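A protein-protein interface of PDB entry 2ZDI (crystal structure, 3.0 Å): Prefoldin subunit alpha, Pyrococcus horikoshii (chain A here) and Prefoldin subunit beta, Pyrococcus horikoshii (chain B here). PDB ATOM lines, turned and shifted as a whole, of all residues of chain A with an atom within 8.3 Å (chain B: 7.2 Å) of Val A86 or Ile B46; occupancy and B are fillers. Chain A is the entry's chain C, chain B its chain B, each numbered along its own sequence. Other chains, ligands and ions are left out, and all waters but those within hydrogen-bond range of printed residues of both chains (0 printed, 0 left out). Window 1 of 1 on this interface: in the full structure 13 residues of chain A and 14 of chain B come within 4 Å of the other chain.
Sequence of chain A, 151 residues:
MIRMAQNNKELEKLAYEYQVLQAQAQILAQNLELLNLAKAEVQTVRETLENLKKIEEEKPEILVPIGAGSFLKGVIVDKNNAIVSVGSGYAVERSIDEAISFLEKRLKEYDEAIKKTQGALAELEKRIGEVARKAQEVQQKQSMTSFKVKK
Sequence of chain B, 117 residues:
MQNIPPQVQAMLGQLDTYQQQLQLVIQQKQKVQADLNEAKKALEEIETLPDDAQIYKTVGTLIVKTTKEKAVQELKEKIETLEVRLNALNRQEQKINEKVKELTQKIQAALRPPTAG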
ATOM      1  N   ILE A  83      11.835  22.958  -1.490  1.00  0.00           N
ATOM      2  CA  ILE A  83      12.321  23.325  -2.819  1.00  0.00           C
ATOM      3  C   ILE A  83      13.826  23.577  -2.785  1.00  0.00           C
ATOM      4  O   ILE A  83      14.297  24.544  -2.188  1.00  0.00           O
ATOM      5  CB  ILE A  83      11.611  24.569  -3.397  1.00  0.00           C
ATOM      6  CG1 ILE A  83      10.156  24.254  -3.736  1.00  0.00           C
ATOM      7  CG2 ILE A  83      12.317  25.044  -4.652  1.00  0.00           C
ATOM      8  CD1 ILE A  83       9.206  24.421  -2.582  1.00  0.00           C
ATOM      9  N   VAL A  84      14.577  22.690  -3.426  1.00  0.00           N
ATOM     10  CA  VAL A  84      16.022  22.817  -3.479  1.00  0.00           C
ATOM     11  C   VAL A  84      16.459  23.209  -4.882  1.00  0.00           C
ATOM     12  O   VAL A  84      15.957  22.675  -5.871  1.00  0.00           O
ATOM     13  CB  VAL A  84      16.709  21.504  -3.084  1.00  0.00           C
ATOM     14  CG1 VAL A  84      18.173  21.750  -2.764  1.00  0.00           C
ATOM     15  CG2 VAL A  84      16.005  20.889  -1.894  1.00  0.00           C
ATOM     16  N   SER A  85      17.397  24.144  -4.965  1.00  0.00           N
ATOM     17  CA  SER A  85      17.856  24.639  -6.251  1.00  0.00           C
ATOM     18  C   SER A  85      18.678  23.603  -7.020  1.00  0.00           C
ATOM     19  O   SER A  85      19.697  23.117  -6.532  1.00  0.00           O
ATOM     20  CB  SER A  85      18.663  25.922  -6.064  1.00  0.00           C
ATOM     21  OG  SER A  85      19.002  26.487  -7.316  1.00  0.00           O
ATOM     22  N   VAL A  86      18.226  23.277  -8.229  1.00  0.00           N
ATOM     23  CA  VAL A  86      18.917  22.316  -9.079  1.00  0.00           C
ATOM     24  C   VAL A  86      19.971  23.004  -9.945  1.00  0.00           C
ATOM     25  O   VAL A  86      20.797  22.340 -10.570  1.00  0.00           O
ATOM     26  CB  VAL A  86      17.929  21.542  -9.979  1.00  0.00           C
ATOM     27  N   GLY A  87      19.939  24.333  -9.972  1.00  0.00           N
ATOM     28  CA  GLY A  87      20.880  25.111 -10.762  1.00  0.00           C
ATOM     29  C   GLY A  87      20.283  25.625 -12.057  1.00  0.00           C
ATOM     30  O   GLY A  87      19.279  25.107 -12.538  1.00  0.00           O
ATOM     31  N   SER A  88      20.899  26.663 -12.613  1.00  0.00           N
ATOM     32  CA  SER A  88      20.545  27.173 -13.941  1.00  0.00           C
ATOM     33  C   SER A  88      19.115  27.719 -14.087  1.00  0.00           C
ATOM     34  O   SER A  88      18.515  27.618 -15.159  1.00  0.00           O
ATOM     35  CB  SER A  88      20.819  26.109 -15.014  1.00  0.00           C
ATOM     36  OG  SER A  88      20.903  26.684 -16.306  1.00  0.00           O
ATOM     37  N   GLY A  89      18.585  28.305 -13.014  1.00  0.00           N
ATOM     38  CA  GLY A  89      17.269  28.921 -13.040  1.00  0.00           C
ATOM     39  C   GLY A  89      16.139  27.999 -12.621  1.00  0.00           C
ATOM     40  O   GLY A  89      14.963  28.319 -12.805  1.00  0.00           O
ATOM     41  N   TYR A  90      16.495  26.855 -12.047  1.00  0.00           N
ATOM     42  CA  TYR A  90      15.515  25.834 -11.693  1.00  0.00           C
ATOM     43  C   TYR A  90      15.718  25.285 -10.280  1.00  0.00           C
ATOM     44  O   TYR A  90      16.844  25.181  -9.795  1.00  0.00           O
ATOM     45  CB  TYR A  90      15.567  24.687 -12.707  1.00  0.00           C
ATOM     46  CG  TYR A  90      15.094  25.059 -14.097  1.00  0.00           C
ATOM     47  CD1 TYR A  90      13.741  25.095 -14.404  1.00  0.00           C
ATOM     48  CD2 TYR A  90      16.001  25.366 -15.107  1.00  0.00           C
ATOM     49  CE1 TYR A  90      13.299  25.427 -15.672  1.00  0.00           C
ATOM     50  CE2 TYR A  90      15.568  25.703 -16.379  1.00  0.00           C
ATOM     51  CZ  TYR A  90      14.215  25.730 -16.654  1.00  0.00           C
ATOM     52  OH  TYR A  90      13.773  26.065 -17.913  1.00  0.00           O
ATOM     53  N   ALA A  91      14.618  24.930  -9.625  1.00  0.00           N
ATOM     54  CA  ALA A  91      14.671  24.290  -8.315  1.00  0.00           C
ATOM     55  C   ALA A  91      13.538  23.282  -8.199  1.00  0.00           C
ATOM     56  O   ALA A  91      12.417  23.553  -8.615  1.00  0.00           O
ATOM     57  CB  ALA A  91      14.581  25.323  -7.205  1.00  0.00           C
ATOM     58  N   VAL A  92      13.832  22.117  -7.636  1.00  0.00           N
ATOM     59  CA  VAL A  92      12.838  21.061  -7.549  1.00  0.00           C
ATOM     60  C   VAL A  92      12.364  20.847  -6.120  1.00  0.00           C
ATOM     61  O   VAL A  92      13.148  20.918  -5.172  1.00  0.00           O
ATOM     62  CB  VAL A  92      13.385  19.739  -8.106  1.00  0.00           C
ATOM     63  CG1 VAL A  92      13.903  19.944  -9.515  1.00  0.00           C
ATOM     64  CG2 VAL A  92      14.491  19.211  -7.213  1.00  0.00           C
ATOM     65  N   GLU A  93      11.070  20.591  -5.975  1.00  0.00           N
ATOM     66  CA  GLU A  93      10.503  20.244  -4.681  1.00  0.00           C
ATOM     67  C   GLU A  93      10.782  18.779  -4.373  1.00  0.00           C
ATOM     68  O   GLU A  93      10.557  17.905  -5.208  1.00  0.00           O
ATOM     69  CB  GLU A  93       9.002  20.515  -4.668  1.00  0.00           C
ATOM     70  CG  GLU A  93       8.303  20.066  -3.404  1.00  0.00           C
ATOM     71  CD  GLU A  93       6.799  20.207  -3.501  1.00  0.00           C
ATOM     72  OE1 GLU A  93       6.325  21.311  -3.845  1.00  0.00           O
ATOM     73  OE2 GLU A  93       6.091  19.214  -3.233  1.00  0.00           O
ATOM     74  N   ARG A  94      11.280  18.520  -3.171  1.00  0.00           N
ATOM     75  CA  ARG A  94      11.674  17.179  -2.768  1.00  0.00           C
ATOM     76  C   ARG A  94      11.097  16.880  -1.404  1.00  0.00           C
ATOM     77  O   ARG A  94      10.691  17.790  -0.691  1.00  0.00           O
ATOM     78  CB  ARG A  94      13.193  17.099  -2.663  1.00  0.00           C
ATOM     79  CG  ARG A  94      13.935  17.469  -3.923  1.00  0.00           C
ATOM     80  CD  ARG A  94      14.211  16.243  -4.761  1.00  0.00           C
ATOM     81  NE  ARG A  94      15.347  16.459  -5.650  1.00  0.00           N
ATOM     82  CZ  ARG A  94      16.148  15.496  -6.090  1.00  0.00           C
ATOM     83  NH1 ARG A  94      17.159  15.792  -6.897  1.00  0.00           N
ATOM     84  NH2 ARG A  94      15.944  14.236  -5.715  1.00  0.00           N
ATOM     85  N   PHE A 102      20.241  15.372  -1.430  1.00  0.00           N
ATOM     86  CA  PHE A 102      20.797  16.183  -2.509  1.00  0.00           C
ATOM     87  C   PHE A 102      21.764  17.224  -1.958  1.00  0.00           C
ATOM     88  O   PHE A 102      22.777  17.535  -2.581  1.00  0.00           O
ATOM     89  CB  PHE A 102      19.686  16.860  -3.316  1.00  0.00           C
ATOM     90  CG  PHE A 102      20.188  17.868  -4.313  1.00  0.00           C
ATOM     91  CD1 PHE A 102      20.103  19.227  -4.048  1.00  0.00           C
ATOM     92  CD2 PHE A 102      20.754  17.459  -5.509  1.00  0.00           C
ATOM     93  CE1 PHE A 102      20.568  20.163  -4.962  1.00  0.00           C
ATOM     94  CE2 PHE A 102      21.222  18.390  -6.426  1.00  0.00           C
ATOM     95  CZ  PHE A 102      21.129  19.743  -6.151  1.00  0.00           C
ATOM     96  N   ARG A 106      25.823  17.890  -2.719  1.00  0.00           N
ATOM     97  CA  ARG A 106      26.463  19.167  -3.031  1.00  0.00           C
ATOM     98  C   ARG A 106      27.472  19.533  -1.948  1.00  0.00           C
ATOM     99  O   ARG A 106      28.416  20.284  -2.187  1.00  0.00           O
ATOM    100  CB  ARG A 106      25.431  20.286  -3.196  1.00  0.00           C
ATOM    101  CG  ARG A 106      24.902  20.447  -4.615  1.00  0.00           C
ATOM    102  CD  ARG A 106      24.944  21.909  -5.030  1.00  0.00           C
ATOM    103  NE  ARG A 106      26.244  22.503  -4.721  1.00  0.00           N
ATOM    104  CZ  ARG A 106      27.267  22.555  -5.570  1.00  0.00           C
ATOM    105  NH1 ARG A 106      28.417  23.107  -5.199  1.00  0.00           N
ATOM    106  NH2 ARG A 106      27.142  22.059  -6.793  1.00  0.00           N
ATOM    107  N   GLU B  38      26.566  24.529 -16.038  1.00  0.00           N
ATOM    108  CA  GLU B  38      25.469  24.714 -15.101  1.00  0.00           C
ATOM    109  C   GLU B  38      24.151  24.189 -15.658  1.00  0.00           C
ATOM    110  O   GLU B  38      23.356  23.592 -14.927  1.00  0.00           O
ATOM    111  CB  GLU B  38      25.331  26.194 -14.735  1.00  0.00           C
ATOM    112  CG  GLU B  38      24.506  26.448 -13.484  1.00  0.00           C
ATOM    113  CD  GLU B  38      24.145  27.910 -13.314  1.00  0.00           C
ATOM    114  OE1 GLU B  38      24.657  28.741 -14.097  1.00  0.00           O
ATOM    115  OE2 GLU B  38      23.347  28.225 -12.402  1.00  0.00           O
ATOM    116  N   ALA B  39      23.927  24.413 -16.951  1.00  0.00           N
ATOM    117  CA  ALA B  39      22.696  23.988 -17.613  1.00  0.00           C
ATOM    118  C   ALA B  39      22.625  22.469 -17.722  1.00  0.00           C
ATOM    119  O   ALA B  39      21.587  21.862 -17.454  1.00  0.00           O
ATOM    120  CB  ALA B  39      22.584  24.630 -18.989  1.00  0.00           C
ATOM    121  N   LYS B  40      23.740  21.862 -18.114  1.00  0.00           N
ATOM    122  CA  LYS B  40      23.814  20.413 -18.251  1.00  0.00           C
ATOM    123  C   LYS B  40      23.566  19.692 -16.927  1.00  0.00           C
ATOM    124  O   LYS B  40      22.767  18.755 -16.870  1.00  0.00           O
ATOM    125  CB  LYS B  40      25.157  19.990 -18.852  1.00  0.00           C
ATOM    126  CG  LYS B  40      25.217  20.092 -20.370  1.00  0.00           C
ATOM    127  CD  LYS B  40      26.478  19.441 -20.930  1.00  0.00           C
ATOM    128  CE  LYS B  40      26.399  19.271 -22.444  1.00  0.00           C
ATOM    129  NZ  LYS B  40      27.599  18.593 -23.013  1.00  0.00           N
ATOM    130  N   LYS B  41      24.247  20.132 -15.869  1.00  0.00           N
ATOM    131  CA  LYS B  41      24.097  19.508 -14.553  1.00  0.00           C
ATOM    132  C   LYS B  41      22.674  19.651 -14.017  1.00  0.00           C
ATOM    133  O   LYS B  41      22.164  18.767 -13.321  1.00  0.00           O
ATOM    134  CB  LYS B  41      25.092  20.088 -13.542  1.00  0.00           C
ATOM    135  CG  LYS B  41      25.165  19.288 -12.239  1.00  0.00           C
ATOM    136  CD  LYS B  41      25.577  20.144 -11.044  1.00  0.00           C
ATOM    137  CE  LYS B  41      25.398  19.380  -9.734  1.00  0.00           C
ATOM    138  NZ  LYS B  41      25.352  20.278  -8.545  1.00  0.00           N
ATOM    139  N   ALA B  42      22.043  20.776 -14.340  1.00  0.00           N
ATOM    140  CA  ALA B  42      20.659  21.017 -13.957  1.00  0.00           C
ATOM    141  C   ALA B  42      19.758  20.019 -14.670  1.00  0.00           C
ATOM    142  O   ALA B  42      18.870  19.423 -14.061  1.00  0.00           O
ATOM    143  CB  ALA B  42      20.254  22.438 -14.301  1.00  0.00           C
ATOM    144  N   LEU B  43      20.004  19.831 -15.961  1.00  0.00           N
ATOM    145  CA  LEU B  43      19.180  18.942 -16.764  1.00  0.00           C
ATOM    146  C   LEU B  43      19.230  17.512 -16.247  1.00  0.00           C
ATOM    147  O   LEU B  43      18.191  16.882 -16.042  1.00  0.00           O
ATOM    148  CB  LEU B  43      19.603  18.988 -18.232  1.00  0.00           C
ATOM    149  CG  LEU B  43      18.801  18.088 -19.176  1.00  0.00           C
ATOM    150  CD1 LEU B  43      17.308  18.271 -18.971  1.00  0.00           C
ATOM    151  CD2 LEU B  43      19.181  18.370 -20.609  1.00  0.00           C
ATOM    152  N   GLU B  44      20.437  17.001 -16.035  1.00  0.00           N
ATOM    153  CA  GLU B  44      20.588  15.622 -15.588  1.00  0.00           C
ATOM    154  C   GLU B  44      19.956  15.407 -14.215  1.00  0.00           C
ATOM    155  O   GLU B  44      19.617  14.284 -13.851  1.00  0.00           O
ATOM    156  CB  GLU B  44      22.061  15.189 -15.602  1.00  0.00           C
ATOM    157  CG  GLU B  44      22.961  15.915 -14.615  1.00  0.00           C
ATOM    158  CD  GLU B  44      24.440  15.655 -14.866  1.00  0.00           C
ATOM    159  OE1 GLU B  44      25.131  15.206 -13.925  1.00  0.00           O
ATOM    160  OE2 GLU B  44      24.912  15.895 -16.001  1.00  0.00           O
ATOM    161  N   GLU B  45      19.783  16.496 -13.473  1.00  0.00           N
ATOM    162  CA  GLU B  45      19.162  16.446 -12.156  1.00  0.00           C
ATOM    163  C   GLU B  45      17.641  16.336 -12.258  1.00  0.00           C
ATOM    164  O   GLU B  45      17.000  15.678 -11.441  1.00  0.00           O
ATOM    165  CB  GLU B  45      19.544  17.687 -11.349  1.00  0.00           C
ATOM    166  CG  GLU B  45      19.253  17.562  -9.865  1.00  0.00           C
ATOM    167  CD  GLU B  45      19.987  16.395  -9.234  1.00  0.00           C
ATOM    168  OE1 GLU B  45      19.343  15.608  -8.508  1.00  0.00           O
ATOM    169  OE2 GLU B  45      21.206  16.258  -9.473  1.00  0.00           O
ATOM    170  N   ILE B  46      17.076  16.989 -13.267  1.00  0.00           N
ATOM    171  CA  ILE B  46      15.635  16.978 -13.501  1.00  0.00           C
ATOM    172  C   ILE B  46      15.164  15.655 -14.110  1.00  0.00           C
ATOM    173  O   ILE B  46      14.045  15.205 -13.852  1.00  0.00           O
ATOM    174  CB  ILE B  46      15.206  18.150 -14.423  1.00  0.00           C
ATOM    175  CG1 ILE B  46      14.928  19.412 -13.606  1.00  0.00           C
ATOM    176  CG2 ILE B  46      13.966  17.790 -15.223  1.00  0.00           C
ATOM    177  CD1 ILE B  46      16.161  20.163 -13.206  1.00  0.00           C
ATOM    178  N   GLU B  47      16.025  15.040 -14.916  1.00  0.00           N
ATOM    179  CA  GLU B  47      15.704  13.781 -15.582  1.00  0.00           C
ATOM    180  C   GLU B  47      15.382  12.660 -14.592  1.00  0.00           C
ATOM    181  O   GLU B  47      14.631  11.742 -14.910  1.00  0.00           O
ATOM    182  CB  GLU B  47      16.862  13.352 -16.485  1.00  0.00           C
ATOM    183  CG  GLU B  47      17.121  14.275 -17.668  1.00  0.00           C
ATOM    184  CD  GLU B  47      16.178  14.025 -18.838  1.00  0.00           C
ATOM    185  OE1 GLU B  47      14.984  13.736 -18.600  1.00  0.00           O
ATOM    186  OE2 GLU B  47      16.633  14.121 -20.001  1.00  0.00           O
ATOM    187  N   THR B  48      15.950  12.752 -13.393  1.00  0.00           N
ATOM    188  CA  THR B  48      15.792  11.726 -12.364  1.00  0.00           C
ATOM    189  C   THR B  48      14.452  11.832 -11.641  1.00  0.00           C
ATOM    190  O   THR B  48      14.176  11.075 -10.707  1.00  0.00           O
ATOM    191  CB  THR B  48      16.905  11.837 -11.301  1.00  0.00           C
ATOM    192  OG1 THR B  48      18.098  12.358 -11.897  1.00  0.00           O
ATOM    193  CG2 THR B  48      17.196  10.475 -10.678  1.00  0.00           C
ATOM    194  N   LEU B  49      13.620  12.770 -12.068  1.00  0.00           N
ATOM    195  CA  LEU B  49      12.388  13.047 -11.348  1.00  0.00           C
ATOM    196  C   LEU B  49      11.185  12.378 -11.987  1.00  0.00           C
ATOM    197  O   LEU B  49      11.145  12.191 -13.206  1.00  0.00           O
ATOM    198  CB  LEU B  49      12.151  14.555 -11.251  1.00  0.00           C
ATOM    199  CG  LEU B  49      13.322  15.385 -10.729  1.00  0.00           C
ATOM    200  CD1 LEU B  49      12.877  16.811 -10.485  1.00  0.00           C
ATOM    201  CD2 LEU B  49      13.889  14.771  -9.456  1.00  0.00           C
ATOM    202  N   PRO B  50      10.201  12.001 -11.160  1.00  0.00           N
ATOM    203  CA  PRO B  50       8.899  11.538 -11.638  1.00  0.00           C
ATOM    204  C   PRO B  50       8.255  12.649 -12.450  1.00  0.00           C
ATOM    205  O   PRO B  50       8.461  13.820 -12.143  1.00  0.00           O
ATOM    206  CB  PRO B  50       8.113  11.314 -10.340  1.00  0.00           C
ATOM    207  CG  PRO B  50       8.859  12.118  -9.306  1.00  0.00           C
ATOM    208  CD  PRO B  50      10.282  11.927  -9.691  1.00  0.00           C
ATOM    209  N   ASP B  51       7.495  12.293 -13.477  1.00  0.00           N
ATOM    210  CA  ASP B  51       6.850  13.293 -14.316  1.00  0.00           C
ATOM    211  C   ASP B  51       6.025  14.255 -13.463  1.00  0.00           C
ATOM    212  O   ASP B  51       5.876  15.431 -13.799  1.00  0.00           O
ATOM    213  CB  ASP B  51       5.967  12.610 -15.360  1.00  0.00           C
ATOM    214  CG  ASP B  51       6.675  11.465 -16.063  1.00  0.00           C
ATOM    215  OD1 ASP B  51       5.992  10.502 -16.468  1.00  0.00           O
ATOM    216  OD2 ASP B  51       7.916  11.524 -16.205  1.00  0.00           O
ATOM    217  N   ALA B  53       6.774  15.335 -10.560  1.00  0.00           N
ATOM    218  CA  ALA B  53       7.629  16.163  -9.717  1.00  0.00           C
ATOM    219  C   ALA B  53       7.315  17.634  -9.939  1.00  0.00           C
ATOM    220  O   ALA B  53       7.138  18.073 -11.080  1.00  0.00           O
ATOM    221  CB  ALA B  53       9.092  15.887 -10.002  1.00  0.00           C
ATOM    222  N   ILE B  55       8.456  21.233 -10.122  1.00  0.00           N
ATOM    223  CA  ILE B  55       9.662  22.032 -10.281  1.00  0.00           C
ATOM    224  C   ILE B  55       9.328  23.525 -10.390  1.00  0.00           C
ATOM    225  O   ILE B  55       8.275  23.904 -10.902  1.00  0.00           O
ATOM    226  CB  ILE B  55      10.545  21.529 -11.467  1.00  0.00           C
ATOM    227  CG1 ILE B  55      10.310  22.351 -12.731  1.00  0.00           C
ATOM    228  CG2 ILE B  55      10.343  20.036 -11.715  1.00  0.00           C
ATOM    229  CD1 ILE B  55      11.313  23.466 -12.905  1.00  0.00           C
ATOM    230  N   TYR B  56      10.229  24.362  -9.877  1.00  0.00           N
ATOM    231  CA  TYR B  56      10.034  25.810  -9.849  1.00  0.00           C
ATOM    232  C   TYR B  56      11.101  26.540 -10.664  1.00  0.00           C
ATOM    233  O   TYR B  56      12.296  26.400 -10.416  1.00  0.00           O
ATOM    234  CB  TYR B  56      10.002  26.324  -8.401  1.00  0.00           C
ATOM    235  CG  TYR B  56       8.758  25.895  -7.654  1.00  0.00           C
ATOM    236  CD1 TYR B  56       7.637  26.711  -7.607  1.00  0.00           C
ATOM    237  CD2 TYR B  56       8.693  24.661  -7.020  1.00  0.00           C
ATOM    238  CE1 TYR B  56       6.488  26.317  -6.938  1.00  0.00           C
ATOM    239  CE2 TYR B  56       7.548  24.258  -6.349  1.00  0.00           C
ATOM    240  CZ  TYR B  56       6.448  25.089  -6.311  1.00  0.00           C
ATOM    241  OH  TYR B  56       5.305  24.694  -5.647  1.00  0.00           O
ATOM    242  N   THR B  67       6.817  22.495 -15.004  1.00  0.00           N
ATOM    243  CA  THR B  67       6.770  21.042 -14.890  1.00  0.00           C
ATOM    244  C   THR B  67       8.016  20.366 -15.455  1.00  0.00           C
ATOM    245  O   THR B  67       8.724  20.946 -16.274  1.00  0.00           O
ATOM    246  CB  THR B  67       5.527  20.474 -15.589  1.00  0.00           C
ATOM    247  OG1 THR B  67       5.566  19.043 -15.541  1.00  0.00           O
ATOM    248  CG2 THR B  67       5.478  20.929 -17.032  1.00  0.00           C
ATOM    249  N   LYS B  68       8.278  19.139 -15.002  1.00  0.00           N
ATOM    250  CA  LYS B  68       9.424  18.367 -15.472  1.00  0.00           C
ATOM    251  C   LYS B  68       9.461  18.354 -16.993  1.00  0.00           C
ATOM    252  O   LYS B  68      10.495  18.618 -17.602  1.00  0.00           O
ATOM    253  CB  LYS B  68       9.359  16.932 -14.943  1.00  0.00           C
ATOM    254  CG  LYS B  68      10.597  16.102 -15.267  1.00  0.00           C
ATOM    255  CD  LYS B  68      10.308  14.606 -15.234  1.00  0.00           C
ATOM    256  CE  LYS B  68      11.442  13.807 -15.868  1.00  0.00           C
ATOM    257  NZ  LYS B  68      11.060  12.394 -16.153  1.00  0.00           N
ATOM    258  N   GLU B  69       8.314  18.047 -17.592  1.00  0.00           N
ATOM    259  CA  GLU B  69       8.157  18.045 -19.042  1.00  0.00           C
ATOM    260  C   GLU B  69       8.658  19.346 -19.658  1.00  0.00           C
ATOM    261  O   GLU B  69       9.572  19.343 -20.484  1.00  0.00           O
ATOM    262  CB  GLU B  69       6.686  17.842 -19.410  1.00  0.00           C
ATOM    263  CG  GLU B  69       6.355  18.236 -20.844  1.00  0.00           C
ATOM    264  CD  GLU B  69       4.890  18.593 -21.037  1.00  0.00           C
ATOM    265  OE1 GLU B  69       4.049  18.098 -20.256  1.00  0.00           O
ATOM    266  OE2 GLU B  69       4.581  19.370 -21.969  1.00  0.00           O
ATOM    267  N   ALA B  71      10.257  21.869 -18.190  1.00  0.00           N
ATOM    268  CA  ALA B  71      11.601  22.178 -17.715  1.00  0.00           C
ATOM    269  C   ALA B  71      12.680  21.504 -18.554  1.00  0.00           C
ATOM    270  O   ALA B  71      13.696  22.117 -18.879  1.00  0.00           O
ATOM    271  CB  ALA B  71      11.744  21.787 -16.258  1.00  0.00           C
ATOM    272  N   VAL B  72      12.450  20.243 -18.907  1.00  0.00           N
ATOM    273  CA  VAL B  72      13.440  19.459 -19.648  1.00  0.00           C
ATOM    274  C   VAL B  72      13.535  19.877 -21.116  1.00  0.00           C
ATOM    275  O   VAL B  72      14.585  19.743 -21.738  1.00  0.00           O
ATOM    276  CB  VAL B  72      13.180  17.937 -19.525  1.00  0.00           C
ATOM    277  CG1 VAL B  72      11.897  17.548 -20.233  1.00  0.00           C
ATOM    278  CG2 VAL B  72      14.348  17.151 -20.083  1.00  0.00           C
ATOM    279  N   GLN B  73      12.435  20.388 -21.663  1.00  0.00           N
ATOM    280  CA  GLN B  73      12.442  20.953 -23.007  1.00  0.00           C
ATOM    281  C   GLN B  73      13.271  22.228 -23.023  1.00  0.00           C
ATOM    282  O   GLN B  73      14.190  22.380 -23.831  1.00  0.00           O
ATOM    283  CB  GLN B  73      11.023  21.293 -23.459  1.00  0.00           C
ATOM    284  CG  GLN B  73      10.105  20.110 -23.693  1.00  0.00           C
ATOM    285  CD  GLN B  73       8.805  20.532 -24.349  1.00  0.00           C
ATOM    286  OE1 GLN B  73       7.724  20.118 -23.936  1.00  0.00           O
ATOM    287  NE2 GLN B  73       8.905  21.379 -25.368  1.00  0.00           N
ATOM    288  N   LEU B  75      15.430  23.290 -20.919  1.00  0.00           N
ATOM    289  CA  LEU B  75      16.820  23.002 -20.587  1.00  0.00           C
ATOM    290  C   LEU B  75      17.589  22.392 -21.752  1.00  0.00           C
ATOM    291  O   LEU B  75      18.752  22.723 -21.974  1.00  0.00           O
ATOM    292  CB  LEU B  75      16.893  22.086 -19.365  1.00  0.00           C
ATOM    293  CG  LEU B  75      16.784  22.778 -18.004  1.00  0.00           C
ATOM    294  CD1 LEU B  75      16.518  21.767 -16.891  1.00  0.00           C
ATOM    295  CD2 LEU B  75      18.045  23.584 -17.723  1.00  0.00           C
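OE2 of Glu B38 is in hydrogen-bond range of N of Ser A88 (2.9 Å). The backbone carbonyl oxygen (O) of Ala A91 sits at hydrogen-bond distance from the backbone NH (N) of Tyr B56 (2.7 Å). OE1 of Glu B45 lies within salt-bridge range of NH1 of Arg A94. The guanidinium group (NH2) of Arg A106 lies close to the side-chain amino group (NZ) of Lys B41 (3.1 Å).
Among the printed residues, merely in contact across the chains: Tyr A90 with Ile B55, Gly A87 with Ala B42, Val A92 with Leu B49, Ser A88 with Ala B39, Tyr A90 with Tyr B56, Tyr A90 with Leu B75, Ala A91 with Ile B55, Ile A83 with Tyr B56, Val A86 with Ala B42, Phe A102 with Glu B45, Ser A88 with Ala B42, Val A86 with Ile B46 and Glu A93 with Tyr B56.
O of Val A84 is in hydrogen-bond range of N of Val A92 (2.8 Å). The backbone carbonyl oxygen (O) of Leu B49 sits at hydrogen-bond distance from the side-chain amino group (NZ) of Lys B68, 3.0 Å away.
Printed residues of chain B within 4 Å of Val A86: Ala B42 and Ile B46. Of the printed residues of chain B, Ile A83 touches Tyr B56. Of the printed residues of chain B, Glu A93 touches Tyr B56 (3.97 Å). Of the printed residues of chain B, Arg A106 touches Lys B41 (3.1 Å). Val B72 touches none of the printed residues of chain A. The nearest residue of chain A that does not touch Ile B46 is Val A92 (4.3 Å).
Of the 14 printed residues of chain A, 11 touch a printed residue of chain B. Printed residues of chain A that touch a printed residue of chain B: Ile A83, Val A86, Gly A87, Ser A88, Tyr A90, Ala A91, Val A92, Glu A93, Arg A94, Phe A102 and Arg A106. Hydrophobic or aromatic side chains of chain A within 4 Å of the printed part of chain B: Ile A83, Val A86, Tyr A90, Val A92 and Phe A102. Among the printed residues, 17 pairs touch across the chains. Among the printed residues, Asp or Glu carboxylates within 4 Å of a Lys or Arg side-chain nitrogen of the other chain: Arg A94 with Glu B45.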
